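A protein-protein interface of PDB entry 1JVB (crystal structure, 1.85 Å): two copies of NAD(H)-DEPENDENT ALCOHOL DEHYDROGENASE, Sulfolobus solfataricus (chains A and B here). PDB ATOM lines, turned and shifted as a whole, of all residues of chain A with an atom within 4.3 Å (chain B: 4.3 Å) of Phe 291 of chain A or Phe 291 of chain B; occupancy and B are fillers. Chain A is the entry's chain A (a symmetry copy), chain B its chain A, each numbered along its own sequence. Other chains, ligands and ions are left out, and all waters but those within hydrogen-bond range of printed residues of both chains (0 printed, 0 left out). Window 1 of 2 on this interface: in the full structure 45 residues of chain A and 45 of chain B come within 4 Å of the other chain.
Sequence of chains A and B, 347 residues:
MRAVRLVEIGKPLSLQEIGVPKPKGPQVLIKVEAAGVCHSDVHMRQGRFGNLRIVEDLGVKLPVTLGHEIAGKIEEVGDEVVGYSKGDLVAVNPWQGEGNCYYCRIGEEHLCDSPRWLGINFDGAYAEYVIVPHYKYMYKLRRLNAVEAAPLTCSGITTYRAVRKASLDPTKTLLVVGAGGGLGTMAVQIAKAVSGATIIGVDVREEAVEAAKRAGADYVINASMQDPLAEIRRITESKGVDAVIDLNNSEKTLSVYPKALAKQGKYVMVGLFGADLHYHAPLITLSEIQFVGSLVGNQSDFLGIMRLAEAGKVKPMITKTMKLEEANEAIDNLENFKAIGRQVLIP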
ATOM      1  N   PRO A 258     -17.637  16.060   7.139  1.00  0.00           N
ATOM      2  CA  PRO A 258     -16.312  15.433   7.173  1.00  0.00           C
ATOM      3  C   PRO A 258     -16.490  13.905   7.005  1.00  0.00           C
ATOM      4  O   PRO A 258     -15.606  13.223   6.536  1.00  0.00           O
ATOM      5  CB  PRO A 258     -15.794  15.804   8.572  1.00  0.00           C
ATOM      6  CG  PRO A 258     -16.330  17.209   8.724  1.00  0.00           C
ATOM      7  CD  PRO A 258     -17.769  17.080   8.188  1.00  0.00           C
ATOM      8  N   TYR A 267     -10.727  18.627   3.356  1.00  0.00           N
ATOM      9  CA  TYR A 267     -11.893  19.359   3.818  1.00  0.00           C
ATOM     10  C   TYR A 267     -11.435  20.844   3.881  1.00  0.00           C
ATOM     11  O   TYR A 267     -10.726  21.253   4.816  1.00  0.00           O
ATOM     12  CB  TYR A 267     -12.286  18.837   5.178  1.00  0.00           C
ATOM     13  CG  TYR A 267     -13.709  19.225   5.539  1.00  0.00           C
ATOM     14  CD1 TYR A 267     -13.997  20.461   6.108  1.00  0.00           C
ATOM     15  CD2 TYR A 267     -14.781  18.352   5.243  1.00  0.00           C
ATOM     16  CE1 TYR A 267     -15.333  20.846   6.380  1.00  0.00           C
ATOM     17  CE2 TYR A 267     -16.105  18.715   5.505  1.00  0.00           C
ATOM     18  CZ  TYR A 267     -16.377  19.962   6.065  1.00  0.00           C
ATOM     19  OH  TYR A 267     -17.686  20.366   6.282  1.00  0.00           O
ATOM     20  N   LEU A 277     -14.190  22.431  15.402  1.00  0.00           N
ATOM     21  CA  LEU A 277     -14.124  21.156  14.720  1.00  0.00           C
ATOM     22  C   LEU A 277     -13.774  20.196  15.862  1.00  0.00           C
ATOM     23  O   LEU A 277     -12.910  20.513  16.695  1.00  0.00           O
ATOM     24  CB  LEU A 277     -12.986  21.180  13.688  1.00  0.00           C
ATOM     25  CG  LEU A 277     -12.569  19.822  13.119  1.00  0.00           C
ATOM     26  CD1 LEU A 277     -13.688  19.259  12.265  1.00  0.00           C
ATOM     27  CD2 LEU A 277     -11.287  19.966  12.299  1.00  0.00           C
ATOM     28  N   TYR A 279     -12.894  16.169  16.057  1.00  0.00           N
ATOM     29  CA  TYR A 279     -12.723  15.004  15.222  1.00  0.00           C
ATOM     30  C   TYR A 279     -11.695  14.097  15.868  1.00  0.00           C
ATOM     31  O   TYR A 279     -10.693  14.584  16.392  1.00  0.00           O
ATOM     32  CB  TYR A 279     -12.265  15.478  13.832  1.00  0.00           C
ATOM     33  CG  TYR A 279     -12.571  14.530  12.732  1.00  0.00           C
ATOM     34  CD1 TYR A 279     -11.685  13.505  12.432  1.00  0.00           C
ATOM     35  CD2 TYR A 279     -13.765  14.620  12.002  1.00  0.00           C
ATOM     36  CE1 TYR A 279     -11.956  12.595  11.446  1.00  0.00           C
ATOM     37  CE2 TYR A 279     -14.051  13.699  11.001  1.00  0.00           C
ATOM     38  CZ  TYR A 279     -13.143  12.695  10.728  1.00  0.00           C
ATOM     39  OH  TYR A 279     -13.379  11.767   9.734  1.00  0.00           O
ATOM     40  N   ILE A 284      -8.022  10.684  11.545  1.00  0.00           N
ATOM     41  CA  ILE A 284      -7.380  11.545  10.579  1.00  0.00           C
ATOM     42  C   ILE A 284      -6.116  10.813  10.133  1.00  0.00           C
ATOM     43  O   ILE A 284      -5.765  10.783   8.970  1.00  0.00           O
ATOM     44  CB  ILE A 284      -6.988  12.909  11.195  1.00  0.00           C
ATOM     45  CG1 ILE A 284      -8.253  13.708  11.533  1.00  0.00           C
ATOM     46  CG2 ILE A 284      -6.044  13.641  10.222  1.00  0.00           C
ATOM     47  CD1 ILE A 284      -7.984  14.988  12.333  1.00  0.00           C
ATOM     48  N   ILE A 289      -6.829  11.972   5.890  1.00  0.00           N
ATOM     49  CA  ILE A 289      -7.584  13.149   5.442  1.00  0.00           C
ATOM     50  C   ILE A 289      -6.850  14.415   5.953  1.00  0.00           C
ATOM     51  O   ILE A 289      -5.920  14.329   6.778  1.00  0.00           O
ATOM     52  CB  ILE A 289      -9.055  13.184   5.951  1.00  0.00           C
ATOM     53  CG1 ILE A 289      -9.095  13.044   7.468  1.00  0.00           C
ATOM     54  CG2 ILE A 289      -9.901  12.079   5.239  1.00  0.00           C
ATOM     55  CD1 ILE A 289     -10.488  13.310   8.038  1.00  0.00           C
ATOM     56  N   GLN A 290      -7.303  15.565   5.463  1.00  0.00           N
ATOM     57  CA  GLN A 290      -6.714  16.863   5.799  1.00  0.00           C
ATOM     58  C   GLN A 290      -7.797  17.889   6.014  1.00  0.00           C
ATOM     59  O   GLN A 290      -8.780  17.941   5.238  1.00  0.00           O
ATOM     60  CB  GLN A 290      -5.847  17.370   4.649  1.00  0.00           C
ATOM     61  CG  GLN A 290      -4.805  16.339   4.165  1.00  0.00           C
ATOM     62  CD  GLN A 290      -3.787  16.899   3.146  1.00  0.00           C
ATOM     63  OE1 GLN A 290      -3.936  18.000   2.647  1.00  0.00           O
ATOM     64  NE2 GLN A 290      -2.745  16.136   2.871  1.00  0.00           N
ATOM     65  N   PHE A 291      -7.643  18.686   7.064  1.00  0.00           N
ATOM     66  CA  PHE A 291      -8.564  19.814   7.299  1.00  0.00           C
ATOM     67  C   PHE A 291      -7.658  20.999   6.978  1.00  0.00           C
ATOM     68  O   PHE A 291      -6.587  21.127   7.602  1.00  0.00           O
ATOM     69  CB  PHE A 291      -9.011  19.819   8.723  1.00  0.00           C
ATOM     70  CG  PHE A 291      -9.990  18.734   9.005  1.00  0.00           C
ATOM     71  CD1 PHE A 291     -11.334  18.893   8.657  1.00  0.00           C
ATOM     72  CD2 PHE A 291      -9.570  17.547   9.575  1.00  0.00           C
ATOM     73  CE1 PHE A 291     -12.237  17.844   8.885  1.00  0.00           C
ATOM     74  CE2 PHE A 291     -10.485  16.497   9.814  1.00  0.00           C
ATOM     75  CZ  PHE A 291     -11.785  16.644   9.471  1.00  0.00           C
ATOM     76  N   VAL A 292      -8.074  21.827   6.007  1.00  0.00           N
ATOM     77  CA  VAL A 292      -7.229  22.912   5.506  1.00  0.00           C
ATOM     78  C   VAL A 292      -7.962  24.240   5.379  1.00  0.00           C
ATOM     79  O   VAL A 292      -9.062  24.288   4.833  1.00  0.00           O
ATOM     80  CB  VAL A 292      -6.590  22.556   4.113  1.00  0.00           C
ATOM     81  CG1 VAL A 292      -5.993  21.106   4.119  1.00  0.00           C
ATOM     82  CG2 VAL A 292      -7.584  22.658   3.017  1.00  0.00           C
ATOM     83  N   PRO B 258      -0.659  22.595  18.546  1.00  0.00           N
ATOM     84  CA  PRO B 258      -1.240  23.265  17.378  1.00  0.00           C
ATOM     85  C   PRO B 258      -1.068  24.793  17.556  1.00  0.00           C
ATOM     86  O   PRO B 258      -1.013  25.530  16.596  1.00  0.00           O
ATOM     87  CB  PRO B 258      -2.715  22.839  17.436  1.00  0.00           C
ATOM     88  CG  PRO B 258      -2.592  21.410  17.912  1.00  0.00           C
ATOM     89  CD  PRO B 258      -1.533  21.517  19.027  1.00  0.00           C
ATOM     90  N   TYR B 267       0.154  20.476  10.577  1.00  0.00           N
ATOM     91  CA  TYR B 267       0.219  19.680  11.789  1.00  0.00           C
ATOM     92  C   TYR B 267       0.031  18.211  11.316  1.00  0.00           C
ATOM     93  O   TYR B 267      -1.094  17.778  11.013  1.00  0.00           O
ATOM     94  CB  TYR B 267      -0.890  20.115  12.715  1.00  0.00           C
ATOM     95  CG  TYR B 267      -0.643  19.659  14.143  1.00  0.00           C
ATOM     96  CD1 TYR B 267      -1.006  18.386  14.566  1.00  0.00           C
ATOM     97  CD2 TYR B 267       0.024  20.508  15.056  1.00  0.00           C
ATOM     98  CE1 TYR B 267      -0.711  17.940  15.878  1.00  0.00           C
ATOM     99  CE2 TYR B 267       0.323  20.086  16.354  1.00  0.00           C
ATOM    100  CZ  TYR B 267      -0.039  18.803  16.758  1.00  0.00           C
ATOM    101  OH  TYR B 267       0.296  18.342  18.022  1.00  0.00           O
ATOM    102  N   LEU B 277      -9.383  15.918  18.313  1.00  0.00           N
ATOM    103  CA  LEU B 277      -8.829  17.229  18.050  1.00  0.00           C
ATOM    104  C   LEU B 277     -10.049  18.138  18.231  1.00  0.00           C
ATOM    105  O   LEU B 277     -11.145  17.808  17.752  1.00  0.00           O
ATOM    106  CB  LEU B 277      -8.334  17.300  16.597  1.00  0.00           C
ATOM    107  CG  LEU B 277      -8.026  18.699  16.063  1.00  0.00           C
ATOM    108  CD1 LEU B 277      -6.817  19.268  16.781  1.00  0.00           C
ATOM    109  CD2 LEU B 277      -7.778  18.644  14.554  1.00  0.00           C
ATOM    110  N   TYR B 279     -10.718  22.178  17.717  1.00  0.00           N
ATOM    111  CA  TYR B 279     -10.061  23.390  17.291  1.00  0.00           C
ATOM    112  C   TYR B 279     -11.094  24.297  16.652  1.00  0.00           C
ATOM    113  O   TYR B 279     -11.955  23.818  15.915  1.00  0.00           O
ATOM    114  CB  TYR B 279      -8.952  23.008  16.297  1.00  0.00           C
ATOM    115  CG  TYR B 279      -7.855  24.001  16.193  1.00  0.00           C
ATOM    116  CD1 TYR B 279      -7.968  25.071  15.317  1.00  0.00           C
ATOM    117  CD2 TYR B 279      -6.708  23.908  16.994  1.00  0.00           C
ATOM    118  CE1 TYR B 279      -6.987  26.022  15.224  1.00  0.00           C
ATOM    119  CE2 TYR B 279      -5.709  24.871  16.910  1.00  0.00           C
ATOM    120  CZ  TYR B 279      -5.855  25.919  16.023  1.00  0.00           C
ATOM    121  OH  TYR B 279      -4.881  26.890  15.896  1.00  0.00           O
ATOM    122  N   ILE B 284      -8.709  28.062  11.758  1.00  0.00           N
ATOM    123  CA  ILE B 284      -8.048  27.277  10.741  1.00  0.00           C
ATOM    124  C   ILE B 284      -8.167  28.075   9.444  1.00  0.00           C
ATOM    125  O   ILE B 284      -7.241  28.179   8.664  1.00  0.00           O
ATOM    126  CB  ILE B 284      -8.721  25.897  10.552  1.00  0.00           C
ATOM    127  CG1 ILE B 284      -8.500  25.037  11.803  1.00  0.00           C
ATOM    128  CG2 ILE B 284      -8.178  25.251   9.263  1.00  0.00           C
ATOM    129  CD1 ILE B 284      -9.296  23.726  11.805  1.00  0.00           C
ATOM    130  N   ILE B 289      -3.952  27.120   8.359  1.00  0.00           N
ATOM    131  CA  ILE B 289      -3.201  25.943   8.811  1.00  0.00           C
ATOM    132  C   ILE B 289      -3.916  24.677   8.273  1.00  0.00           C
ATOM    133  O   ILE B 289      -5.045  24.752   7.751  1.00  0.00           O
ATOM    134  CB  ILE B 289      -3.081  25.829  10.359  1.00  0.00           C
ATOM    135  CG1 ILE B 289      -4.462  25.887  11.003  1.00  0.00           C
ATOM    136  CG2 ILE B 289      -2.130  26.940  10.913  1.00  0.00           C
ATOM    137  CD1 ILE B 289      -4.421  25.542  12.492  1.00  0.00           C
ATOM    138  N   GLN B 290      -3.247  23.540   8.434  1.00  0.00           N
ATOM    139  CA  GLN B 290      -3.744  22.247   7.957  1.00  0.00           C
ATOM    140  C   GLN B 290      -3.474  21.174   8.980  1.00  0.00           C
ATOM    141  O   GLN B 290      -2.370  21.129   9.573  1.00  0.00           O
ATOM    142  CB  GLN B 290      -3.016  21.833   6.681  1.00  0.00           C
ATOM    143  CG  GLN B 290      -3.022  22.924   5.589  1.00  0.00           C
ATOM    144  CD  GLN B 290      -2.472  22.456   4.222  1.00  0.00           C
ATOM    145  OE1 GLN B 290      -1.917  21.378   4.103  1.00  0.00           O
ATOM    146  NE2 GLN B 290      -2.661  23.268   3.199  1.00  0.00           N
ATOM    147  N   PHE B 291      -4.470  20.329   9.212  1.00  0.00           N
ATOM    148  CA  PHE B 291      -4.281  19.158  10.089  1.00  0.00           C
ATOM    149  C   PHE B 291      -4.305  18.024   9.068  1.00  0.00           C
ATOM    150  O   PHE B 291      -5.298  17.901   8.326  1.00  0.00           O
ATOM    151  CB  PHE B 291      -5.408  19.062  11.061  1.00  0.00           C
ATOM    152  CG  PHE B 291      -5.315  20.095  12.129  1.00  0.00           C
ATOM    153  CD1 PHE B 291      -4.457  19.908  13.215  1.00  0.00           C
ATOM    154  CD2 PHE B 291      -6.047  21.264  12.032  1.00  0.00           C
ATOM    155  CE1 PHE B 291      -4.344  20.911  14.189  1.00  0.00           C
ATOM    156  CE2 PHE B 291      -5.939  22.267  13.021  1.00  0.00           C
ATOM    157  CZ  PHE B 291      -5.103  22.093  14.071  1.00  0.00           C
ATOM    158  N   VAL B 292      -3.220  17.235   9.022  1.00  0.00           N
ATOM    159  CA  VAL B 292      -3.059  16.208   7.991  1.00  0.00           C
ATOM    160  C   VAL B 292      -2.604  14.864   8.542  1.00  0.00           C
ATOM    161  O   VAL B 292      -1.664  14.807   9.332  1.00  0.00           O
ATOM    162  CB  VAL B 292      -2.047  16.661   6.874  1.00  0.00           C
ATOM    163  CG1 VAL B 292      -2.341  18.128   6.405  1.00  0.00           C
ATOM    164  CG2 VAL B 292      -0.643  16.582   7.346  1.00  0.00           C
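The backbone NH (N) of Leu 277 of chain B sits at hydrogen-bond distance from the backbone carbonyl oxygen (O) of Tyr 279 of chain A, 2.7 Å away.
The backbone carbonyl oxygen of Phe 291 of chain A lies within hydrogen-bond range of the backbone NH of Phe 291 of chain B (2.8 Å).
The backbone carbonyl oxygen (O) of Tyr 279 of chain B sits at hydrogen-bond distance from the backbone NH (N) of Leu 277 of chain A (2.7 Å).
The backbone carbonyl oxygen (O) of Leu 277 of chain A sits close to the backbone carbonyl oxygen (O) of Leu 277 of chain B.
The backbone carbonyl oxygen (O) of Tyr 267 of chain B is in hydrogen-bond range of the backbone NH (N) of Val 292 of chain B.
The backbone carbonyl oxygen (O) of Gln 290 of chain B sits at hydrogen-bond distance from the backbone NH (N) of Tyr 267 of chain B, 2.8 Å away.
The backbone carbonyl oxygen (O) of Tyr 267 of chain A sits at hydrogen-bond distance from the backbone NH (N) of Val 292 of chain A (3.0 Å).
The backbone carbonyl oxygen (O) of Ile 284 of chain A lies within hydrogen-bond range of the backbone NH (N) of Ile 289 of chain A (3.5 Å).
N of Tyr 267 of chain A lies within hydrogen-bond range of O of Gln 290 of chain A.
N of Ile 289 of chain B sits at hydrogen-bond distance from O of Ile 284 of chain B (3.5 Å).
Among the printed residues, merely in contact across the chains: Phe 291 of chain A with Gln 290 of chain B (3.1 Å), Gln 290 of chain A with Phe 291 of chain B (3.1 Å), Ile 289 of chain A with Val 292 of chain B (3.6 Å), Val 292 of chain A with Ile 289 of chain B (3.6 Å), Gln 290 of chain A with Val 292 of chain B (3.8 Å), Val 292 of chain A with Gln 290 of chain B (3.8 Å), Phe 291 of chain A with Ile 289 of chain B (3.9 Å) and Ile 289 of chain A with Phe 291 of chain B (3.9 Å).
Tyr 267 of chain A touches none of the printed residues of chain B.
Of the printed residues of chain B, Leu 277 of chain A touches Leu 277 (3.4 Å) and Tyr 279 (2.7 Å).
Ile 284 of chain A touches none of the printed residues of chain B.
Phe 291 of chain A touches just these residues of chain B: Ile 289, Gln 290 and Phe 291.
Of the printed residues of chain A, Tyr 279 of chain B touches Leu 277.
Printed residues of chain A within 4 Å of Ile 289 of chain B: Phe 291 (3.9 Å) and Val 292 (3.6 Å).
Of the printed residues of chain A, Gln 290 of chain B touches Phe 291 (3.1 Å) and Val 292 (3.8 Å).
Phe 291 of chain B touches just these residues of chain A: Ile 289 (3.9 Å), Gln 290 (3.1 Å) and Phe 291 (2.8 Å).
The nearest printed residue of chain A that does not touch Phe 291 of chain B is Ile 284 of chain A (4.7 Å).
The nearest printed residue of chain A that does not touch Ile 289 of chain B is Tyr 267 of chain A (7.3 Å).
Hydrophobic or aromatic side chains of chain A that line the printed part of chain B: Leu 277 and Val 292.
Hydrophobic or aromatic side chains of chain B that line the printed part of chain A: Leu 277 and Val 292.
Along chain B the printed residues that touch a printed residue of chain A span positions 277 to 292.
Among the printed residues, no Asp or Glu carboxylate lies within 4 Å of a Lys or Arg side-chain nitrogen of the other chain.
Leu 277 of chain A touches its own counterpart, Leu 277 of chain B.
Ile 289 of chain A touches Phe 291 of chain B, and with the chains exchanged Phe 291 of chain A touches Ile 289 of chain B.
Ile 289 of chain A touches Val 292 of chain B, and with the chains exchanged Val 292 of chain A touches Ile 289 of chain B.
Gln 290 of chain A touches Val 292 of chain B, and with the chains exchanged Val 292 of chain A touches Gln 290 of chain B.
Positions printed for both chains: 258, 267, 277, 279, 284, 289, 290, 291 and 292.
Of the 12 pairs that touch across the chains among the printed residues, 12 have their exchanged pair printed and touching as well.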
